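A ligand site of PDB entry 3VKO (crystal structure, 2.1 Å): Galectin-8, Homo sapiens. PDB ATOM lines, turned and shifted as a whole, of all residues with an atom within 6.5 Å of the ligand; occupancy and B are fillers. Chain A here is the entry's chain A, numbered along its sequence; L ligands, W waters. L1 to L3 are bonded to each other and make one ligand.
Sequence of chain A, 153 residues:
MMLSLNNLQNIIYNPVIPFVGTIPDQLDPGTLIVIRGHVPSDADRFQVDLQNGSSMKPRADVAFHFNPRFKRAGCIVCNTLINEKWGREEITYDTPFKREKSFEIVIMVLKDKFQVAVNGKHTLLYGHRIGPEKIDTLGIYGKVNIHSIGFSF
An oxygen (O5) of LG2 L2 lies within hydrogen-bond range of the side-chain carboxylate of Glu 89 (2.6 Å).
An oxygen (O3) of LG2 L2 lies within hydrogen-bond range of a ring nitrogen (NE2) of His 65 (2.7 Å).
The guanidinium group (NH1) of Arg 59 is in salt-bridge range of an oxygen (O1) of LG3 L3 (2.8 Å).
An oxygen (O5) of LG2 L2 lies within hydrogen-bond range of the side-chain amide nitrogen (ND2) of Asn 79, at 2.8 Å.
An oxygen (O3) of LG2 L2 is in hydrogen-bond range of the guanidinium group of Arg 69.
An oxygen (O2) of LG2 L2 lies within hydrogen-bond range of the guanidinium group (NH2) of Arg 45, at 3.1 Å.
The side-chain amide oxygen of Asn 67 is in hydrogen-bond range of an oxygen (O3) of LG2 L2 (3.1 Å).
An oxygen (O2) of LG3 L3 sits at hydrogen-bond distance from the indole nitrogen (NE1) of Trp 86 (3.2 Å).
NE2 of Gln 47 is in hydrogen-bond range of O1 of LG3 L3 (3.2 Å).
Water W2 lies within hydrogen-bond range of O6 of LIG L1, OE1 of Glu 89 and NH1 of Arg 69.
The backbone carbonyl oxygen (O) of Asn 79 is in hydrogen-bond range of the backbone NH (N) of His 65 (3.0 Å).
The backbone carbonyl oxygen (O) of Gly 87 sits at hydrogen-bond distance from the side-chain amide nitrogen (ND2) of Asn 79.
OD1 of Asn 79 sits close to O of Arg 88.
The guanidinium group (NE) of Arg 69 sits at hydrogen-bond distance from the side-chain amide oxygen (OD1) of Asn 67 (2.7 Å).
The guanidinium group (NH1) of Arg 45 lies within hydrogen-bond range of the side-chain amide oxygen (OD1) of Asn 67 (3.0 Å).
The side-chain amide oxygen (OE1) of Gln 47 is in hydrogen-bond range of the guanidinium group (NH2) of Arg 45, 2.8 Å away.
NE2 of Gln 47 sits at hydrogen-bond distance from OD2 of Asp 49.
O of Tyr 141 lies within hydrogen-bond range of N of Gln 47.
Hydrophobic or aromatic side chains that line the ligand: His 65 and Trp 86.
The nearest printed residue that does not touch the ligand is Val 77 (4.03 Å).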
ATOM      1  N   ARG A  45       2.821 -16.285 -24.415  1.00  0.00           N
ATOM      2  CA  ARG A  45       3.752 -15.212 -24.090  1.00  0.00           C
ATOM      3  C   ARG A  45       4.505 -15.514 -22.808  1.00  0.00           C
ATOM      4  O   ARG A  45       4.158 -16.445 -22.075  1.00  0.00           O
ATOM      5  CB  ARG A  45       2.999 -13.893 -23.891  1.00  0.00           C
ATOM      6  CG  ARG A  45       1.892 -13.975 -22.839  1.00  0.00           C
ATOM      7  CD  ARG A  45       1.399 -12.606 -22.432  1.00  0.00           C
ATOM      8  NE  ARG A  45       2.240 -12.001 -21.401  1.00  0.00           N
ATOM      9  CZ  ARG A  45       2.267 -10.703 -21.126  1.00  0.00           C
ATOM     10  NH1 ARG A  45       1.508  -9.867 -21.823  1.00  0.00           N
ATOM     11  NH2 ARG A  45       3.023 -10.243 -20.146  1.00  0.00           N
ATOM     12  N   GLN A  47       7.569 -13.307 -19.931  1.00  0.00           N
ATOM     13  CA  GLN A  47       8.262 -12.057 -19.675  1.00  0.00           C
ATOM     14  C   GLN A  47       9.412 -12.183 -18.714  1.00  0.00           C
ATOM     15  O   GLN A  47       9.444 -13.054 -17.837  1.00  0.00           O
ATOM     16  CB  GLN A  47       7.277 -11.009 -19.119  1.00  0.00           C
ATOM     17  CG  GLN A  47       6.830 -11.270 -17.662  1.00  0.00           C
ATOM     18  CD  GLN A  47       5.472 -10.670 -17.358  1.00  0.00           C
ATOM     19  OE1 GLN A  47       4.467 -11.084 -17.937  1.00  0.00           O
ATOM     20  NE2 GLN A  47       5.422  -9.699 -16.446  1.00  0.00           N
ATOM     21  N   ASP A  49      11.327  -9.568 -16.245  1.00  0.00           N
ATOM     22  CA  ASP A  49      11.211  -8.225 -15.672  1.00  0.00           C
ATOM     23  C   ASP A  49      12.340  -7.877 -14.699  1.00  0.00           C
ATOM     24  O   ASP A  49      12.589  -8.601 -13.737  1.00  0.00           O
ATOM     25  CB  ASP A  49       9.887  -8.063 -14.910  1.00  0.00           C
ATOM     26  CG  ASP A  49       8.672  -8.341 -15.775  1.00  0.00           C
ATOM     27  OD1 ASP A  49       8.682  -7.978 -16.974  1.00  0.00           O
ATOM     28  OD2 ASP A  49       7.709  -8.904 -15.234  1.00  0.00           O
ATOM     29  N   ARG A  59       2.389  -3.834  -6.250  1.00  0.00           N
ATOM     30  CA  ARG A  59       3.308  -4.510  -7.162  1.00  0.00           C
ATOM     31  C   ARG A  59       4.585  -3.719  -7.367  1.00  0.00           C
ATOM     32  O   ARG A  59       4.547  -2.522  -7.649  1.00  0.00           O
ATOM     33  CB  ARG A  59       2.641  -4.764  -8.509  1.00  0.00           C
ATOM     34  CG  ARG A  59       3.501  -5.553  -9.469  1.00  0.00           C
ATOM     35  CD  ARG A  59       2.759  -5.817 -10.768  1.00  0.00           C
ATOM     36  NE  ARG A  59       3.595  -6.445 -11.788  1.00  0.00           N
ATOM     37  CZ  ARG A  59       3.222  -6.613 -13.059  1.00  0.00           C
ATOM     38  NH1 ARG A  59       4.039  -7.195 -13.914  1.00  0.00           N
ATOM     39  NH2 ARG A  59       2.022  -6.190 -13.455  1.00  0.00           N
ATOM     40  N   HIS A  65      10.649  -4.382 -18.748  1.00  0.00           N
ATOM     41  CA  HIS A  65       9.681  -5.435 -19.046  1.00  0.00           C
ATOM     42  C   HIS A  65       9.947  -5.955 -20.462  1.00  0.00           C
ATOM     43  O   HIS A  65       9.619  -5.284 -21.440  1.00  0.00           O
ATOM     44  CB  HIS A  65       8.263  -4.849 -18.962  1.00  0.00           C
ATOM     45  CG  HIS A  65       7.171  -5.813 -19.305  1.00  0.00           C
ATOM     46  ND1 HIS A  65       6.876  -6.923 -18.543  1.00  0.00           N
ATOM     47  CD2 HIS A  65       6.245  -5.791 -20.294  1.00  0.00           C
ATOM     48  CE1 HIS A  65       5.818  -7.529 -19.037  1.00  0.00           C
ATOM     49  NE2 HIS A  65       5.409  -6.868 -20.100  1.00  0.00           N
ATOM     50  N   ASN A  67       8.836  -8.516 -22.939  1.00  0.00           N
ATOM     51  CA  ASN A  67       7.672  -9.383 -23.152  1.00  0.00           C
ATOM     52  C   ASN A  67       7.455 -10.024 -24.529  1.00  0.00           C
ATOM     53  O   ASN A  67       6.741  -9.468 -25.372  1.00  0.00           O
ATOM     54  CB  ASN A  67       6.419  -8.590 -22.781  1.00  0.00           C
ATOM     55  CG  ASN A  67       5.130  -9.389 -22.901  1.00  0.00           C
ATOM     56  OD1 ASN A  67       4.057  -8.797 -23.012  1.00  0.00           O
ATOM     57  ND2 ASN A  67       5.231 -10.704 -22.857  1.00  0.00           N
ATOM     58  N   ARG A  69       5.649 -12.035 -27.259  1.00  0.00           N
ATOM     59  CA  ARG A  69       4.276 -12.493 -27.472  1.00  0.00           C
ATOM     60  C   ARG A  69       4.253 -13.326 -28.747  1.00  0.00           C
ATOM     61  O   ARG A  69       4.934 -13.003 -29.727  1.00  0.00           O
ATOM     62  CB  ARG A  69       3.330 -11.298 -27.574  1.00  0.00           C
ATOM     63  CG  ARG A  69       3.297 -10.456 -26.299  1.00  0.00           C
ATOM     64  CD  ARG A  69       2.387  -9.230 -26.375  1.00  0.00           C
ATOM     65  NE  ARG A  69       2.348  -8.559 -25.073  1.00  0.00           N
ATOM     66  CZ  ARG A  69       1.567  -7.528 -24.774  1.00  0.00           C
ATOM     67  NH1 ARG A  69       0.730  -7.018 -25.658  1.00  0.00           N
ATOM     68  NH2 ARG A  69       1.621  -7.014 -23.551  1.00  0.00           N
ATOM     69  N   VAL A  77       7.086  -6.939 -26.655  1.00  0.00           N
ATOM     70  CA  VAL A  77       6.636  -5.704 -26.033  1.00  0.00           C
ATOM     71  C   VAL A  77       7.570  -5.362 -24.885  1.00  0.00           C
ATOM     72  O   VAL A  77       7.856  -6.207 -24.038  1.00  0.00           O
ATOM     73  CB  VAL A  77       5.193  -5.848 -25.483  1.00  0.00           C
ATOM     74  CG1 VAL A  77       4.808  -4.586 -24.704  1.00  0.00           C
ATOM     75  CG2 VAL A  77       4.210  -6.082 -26.619  1.00  0.00           C
ATOM     76  N   CYS A  78       8.057  -4.133 -24.882  1.00  0.00           N
ATOM     77  CA  CYS A  78       8.920  -3.652 -23.818  1.00  0.00           C
ATOM     78  C   CYS A  78       8.234  -2.455 -23.180  1.00  0.00           C
ATOM     79  O   CYS A  78       7.631  -1.620 -23.863  1.00  0.00           O
ATOM     80  CB  CYS A  78      10.299  -3.271 -24.361  1.00  0.00           C
ATOM     81  SG  CYS A  78      11.315  -4.681 -24.917  1.00  0.00           S
ATOM     82  N   ASN A  79       8.307  -2.364 -21.852  1.00  0.00           N
ATOM     83  CA  ASN A  79       7.653  -1.271 -21.153  1.00  0.00           C
ATOM     84  C   ASN A  79       8.214  -1.145 -19.757  1.00  0.00           C
ATOM     85  O   ASN A  79       9.096  -1.900 -19.355  1.00  0.00           O
ATOM     86  CB  ASN A  79       6.145  -1.536 -21.085  1.00  0.00           C
ATOM     87  CG  ASN A  79       5.319  -0.250 -20.989  1.00  0.00           C
ATOM     88  OD1 ASN A  79       5.854   0.817 -20.684  1.00  0.00           O
ATOM     89  ND2 ASN A  79       4.016  -0.361 -21.258  1.00  0.00           N
ATOM     90  N   THR A  80       7.697  -0.171 -19.003  1.00  0.00           N
ATOM     91  CA  THR A  80       8.111   0.070 -17.643  1.00  0.00           C
ATOM     92  C   THR A  80       6.878   0.276 -16.785  1.00  0.00           C
ATOM     93  O   THR A  80       5.920   0.950 -17.197  1.00  0.00           O
ATOM     94  CB  THR A  80       8.983   1.336 -17.531  1.00  0.00           C
ATOM     95  OG1 THR A  80      10.247   1.105 -18.166  1.00  0.00           O
ATOM     96  CG2 THR A  80       9.213   1.697 -16.066  1.00  0.00           C
ATOM     97  N   LEU A  81       6.890  -0.318 -15.602  1.00  0.00           N
ATOM     98  CA  LEU A  81       5.771  -0.192 -14.681  1.00  0.00           C
ATOM     99  C   LEU A  81       6.214   0.630 -13.470  1.00  0.00           C
ATOM    100  O   LEU A  81       7.050   0.176 -12.672  1.00  0.00           O
ATOM    101  CB  LEU A  81       5.304  -1.572 -14.211  1.00  0.00           C
ATOM    102  CG  LEU A  81       4.019  -1.600 -13.362  1.00  0.00           C
ATOM    103  CD1 LEU A  81       2.799  -1.377 -14.258  1.00  0.00           C
ATOM    104  CD2 LEU A  81       3.919  -2.939 -12.632  1.00  0.00           C
ATOM    105  N   TRP A  86       1.562   1.099 -16.339  1.00  0.00           N
ATOM    106  CA  TRP A  86       2.428   0.880 -17.492  1.00  0.00           C
ATOM    107  C   TRP A  86       2.605   2.164 -18.288  1.00  0.00           C
ATOM    108  O   TRP A  86       1.676   2.971 -18.395  1.00  0.00           O
ATOM    109  CB  TRP A  86       1.857  -0.214 -18.386  1.00  0.00           C
ATOM    110  CG  TRP A  86       2.000  -1.589 -17.825  1.00  0.00           C
ATOM    111  CD1 TRP A  86       0.998  -2.390 -17.334  1.00  0.00           C
ATOM    112  CD2 TRP A  86       3.215  -2.338 -17.676  1.00  0.00           C
ATOM    113  NE1 TRP A  86       1.521  -3.579 -16.901  1.00  0.00           N
ATOM    114  CE2 TRP A  86       2.878  -3.579 -17.096  1.00  0.00           C
ATOM    115  CE3 TRP A  86       4.557  -2.079 -17.983  1.00  0.00           C
ATOM    116  CZ2 TRP A  86       3.831  -4.559 -16.814  1.00  0.00           C
ATOM    117  CZ3 TRP A  86       5.504  -3.044 -17.706  1.00  0.00           C
ATOM    118  CH2 TRP A  86       5.135  -4.280 -17.129  1.00  0.00           C
ATOM    119  N   GLY A  87       3.802   2.350 -18.826  1.00  0.00           N
ATOM    120  CA  GLY A  87       4.081   3.534 -19.620  1.00  0.00           C
ATOM    121  C   GLY A  87       3.813   3.228 -21.088  1.00  0.00           C
ATOM    122  O   GLY A  87       3.015   2.357 -21.412  1.00  0.00           O
ATOM    123  N   ARG A  88       4.483   3.968 -21.965  1.00  0.00           N
ATOM    124  CA  ARG A  88       4.347   3.801 -23.403  1.00  0.00           C
ATOM    125  C   ARG A  88       5.072   2.541 -23.883  1.00  0.00           C
ATOM    126  O   ARG A  88       6.277   2.388 -23.671  1.00  0.00           O
ATOM    127  CB  ARG A  88       4.921   5.027 -24.116  1.00  0.00           C
ATOM    128  CG  ARG A  88       5.122   4.882 -25.610  1.00  0.00           C
ATOM    129  CD  ARG A  88       6.104   5.950 -26.079  1.00  0.00           C
ATOM    130  NE  ARG A  88       7.332   5.911 -25.293  1.00  0.00           N
ATOM    131  CZ  ARG A  88       8.342   6.763 -25.401  1.00  0.00           C
ATOM    132  NH1 ARG A  88       9.416   6.625 -24.636  1.00  0.00           N
ATOM    133  NH2 ARG A  88       8.281   7.760 -26.281  1.00  0.00           N
ATOM    134  N   GLU A  89       4.339   1.644 -24.527  1.00  0.00           N
ATOM    135  CA  GLU A  89       4.942   0.402 -25.013  1.00  0.00           C
ATOM    136  C   GLU A  89       5.887   0.672 -26.182  1.00  0.00           C
ATOM    137  O   GLU A  89       5.689   1.618 -26.955  1.00  0.00           O
ATOM    138  CB  GLU A  89       3.865  -0.587 -25.468  1.00  0.00           C
ATOM    139  CG  GLU A  89       2.863  -0.984 -24.394  1.00  0.00           C
ATOM    140  CD  GLU A  89       1.989  -2.152 -24.841  1.00  0.00           C
ATOM    141  OE1 GLU A  89       1.572  -2.148 -26.013  1.00  0.00           O
ATOM    142  OE2 GLU A  89       1.722  -3.051 -24.016  1.00  0.00           O
ATOM    143  N   ILE A  91       7.067  -1.591 -29.029  1.00  0.00           N
ATOM    144  CA  ILE A  91       6.896  -2.885 -29.678  1.00  0.00           C
ATOM    145  C   ILE A  91       7.908  -3.154 -30.793  1.00  0.00           C
ATOM    146  O   ILE A  91       8.057  -2.366 -31.724  1.00  0.00           O
ATOM    147  CB  ILE A  91       5.489  -3.012 -30.314  1.00  0.00           C
ATOM    148  CG1 ILE A  91       4.425  -2.393 -29.406  1.00  0.00           C
ATOM    149  CG2 ILE A  91       5.172  -4.475 -30.551  1.00  0.00           C
ATOM    150  CD1 ILE A  91       4.222  -3.127 -28.087  1.00  0.00           C
ATOM    151  N   TYR A 141       8.169 -14.763 -15.726  1.00  0.00           N
ATOM    152  CA  TYR A 141       6.797 -15.277 -15.673  1.00  0.00           C
ATOM    153  C   TYR A 141       6.269 -15.730 -17.047  1.00  0.00           C
ATOM    154  O   TYR A 141       6.876 -15.446 -18.089  1.00  0.00           O
ATOM    155  CB  TYR A 141       5.875 -14.181 -15.134  1.00  0.00           C
ATOM    156  CG  TYR A 141       6.434 -13.427 -13.941  1.00  0.00           C
ATOM    157  CD1 TYR A 141       6.269 -13.895 -12.641  1.00  0.00           C
ATOM    158  CD2 TYR A 141       7.139 -12.230 -14.121  1.00  0.00           C
ATOM    159  CE1 TYR A 141       6.797 -13.201 -11.549  1.00  0.00           C
ATOM    160  CE2 TYR A 141       7.672 -11.530 -13.036  1.00  0.00           C
ATOM    161  CZ  TYR A 141       7.492 -12.024 -11.758  1.00  0.00           C
ATOM    162  OH  TYR A 141       8.022 -11.338 -10.673  1.00  0.00           O
HETATM  163  C1  LIG L   1      -3.799  -2.571 -23.623  1.00  0.00           C
HETATM  164  C2  LIG L   1      -2.527  -2.897 -24.416  1.00  0.00           C
HETATM  165  C3  LIG L   1      -1.920  -4.234 -23.963  1.00  0.00           C
HETATM  166  C4  LIG L   1      -1.728  -4.210 -22.456  1.00  0.00           C
HETATM  167  C5  LIG L   1      -3.066  -3.896 -21.773  1.00  0.00           C
HETATM  168  C6  LIG L   1      -2.991  -3.862 -20.260  1.00  0.00           C
HETATM  169  C7  LIG L   1      -2.209  -2.157 -26.680  1.00  0.00           C
HETATM  170  C8  LIG L   1      -2.500  -0.663 -26.593  1.00  0.00           C
HETATM  171  N1  LIG L   1      -2.847  -2.945 -25.830  1.00  0.00           N
HETATM  172  O1  LIG L   1      -4.197  -1.285 -23.946  1.00  0.00           O
HETATM  173  O2  LIG L   1      -0.668  -4.435 -24.591  1.00  0.00           O
HETATM  174  O3  LIG L   1      -1.224  -5.481 -22.011  1.00  0.00           O
HETATM  175  O4  LIG L   1      -3.543  -2.614 -22.221  1.00  0.00           O
HETATM  176  O5  LIG L   1      -2.098  -2.853 -19.805  1.00  0.00           O
HETATM  177  O6  LIG L   1      -1.394  -2.574 -27.510  1.00  0.00           O
HETATM  178  C1  LG2 L   2      -0.297  -5.418 -20.980  1.00  0.00           C
HETATM  179  C2  LG2 L   2      -0.093  -6.809 -20.408  1.00  0.00           C
HETATM  180  C3  LG2 L   2       0.981  -6.774 -19.317  1.00  0.00           C
HETATM  181  C4  LG2 L   2       2.255  -6.127 -19.852  1.00  0.00           C
HETATM  182  C5  LG2 L   2       1.927  -4.761 -20.459  1.00  0.00           C
HETATM  183  C6  LG2 L   2       3.129  -4.068 -21.080  1.00  0.00           C
HETATM  184  O1  LG2 L   2      -1.314  -7.278 -19.859  1.00  0.00           O
HETATM  185  O2  LG2 L   2       1.251  -8.111 -18.866  1.00  0.00           O
HETATM  186  O3  LG2 L   2       2.843  -6.969 -20.838  1.00  0.00           O
HETATM  187  O4  LG2 L   2       0.934  -4.908 -21.496  1.00  0.00           O
HETATM  188  O5  LG2 L   2       2.756  -2.831 -21.661  1.00  0.00           O
HETATM  189  C1  LG3 L   3       1.597  -7.633 -16.564  1.00  0.00           C
HETATM  190  C2  LG3 L   3       0.837  -8.457 -17.588  1.00  0.00           C
HETATM  191  C3  LG3 L   3       1.096  -9.952 -17.358  1.00  0.00           C
HETATM  192  C4  LG3 L   3       0.425 -10.460 -16.079  1.00  0.00           C
HETATM  193  C5  LG3 L   3      -1.046 -10.038 -16.026  1.00  0.00           C
HETATM  194  C6  LG3 L   3      -1.134  -8.518 -16.203  1.00  0.00           C
HETATM  195  C7  LG3 L   3      -2.578  -8.042 -16.123  1.00  0.00           C
HETATM  196  C8  LG3 L   3      -2.689  -6.585 -16.559  1.00  0.00           C
HETATM  197  C9  LG3 L   3      -4.094  -6.057 -16.332  1.00  0.00           C
HETATM  198  C10 LG3 L   3      -2.588 -11.319 -14.698  1.00  0.00           C
HETATM  199  C11 LG3 L   3      -3.729 -11.068 -13.727  1.00  0.00           C
HETATM  200  N1  LG3 L   3      -1.606 -10.420 -14.745  1.00  0.00           N
HETATM  201  O1  LG3 L   3       2.736  -8.012 -16.213  1.00  0.00           O
HETATM  202  O2  LG3 L   3       1.064  -6.595 -16.110  1.00  0.00           O
HETATM  203  O3  LG3 L   3       0.504 -11.872 -16.040  1.00  0.00           O
HETATM  204  O4  LG3 L   3      -0.564  -8.159 -17.485  1.00  0.00           O
HETATM  205  O5  LG3 L   3      -3.403  -8.848 -16.949  1.00  0.00           O
HETATM  206  O6  LG3 L   3      -1.753  -5.795 -15.848  1.00  0.00           O
HETATM  207  O7  LG3 L   3      -4.214  -4.756 -16.889  1.00  0.00           O
HETATM  208  O8  LG3 L   3      -2.611 -12.328 -15.412  1.00  0.00           O
HETATM  209  O   HOH W   1      -2.593  -7.831 -24.130  1.00  0.00           O
HETATM  210  O   HOH W   2       0.299  -4.455 -26.999  1.00  0.00           O
HETATM  211  O   HOH W   3       1.176 -13.307 -13.750  1.00  0.00           O
HETATM  212  O   HOH W   4      -0.302  -9.533 -12.614  1.00  0.00           O
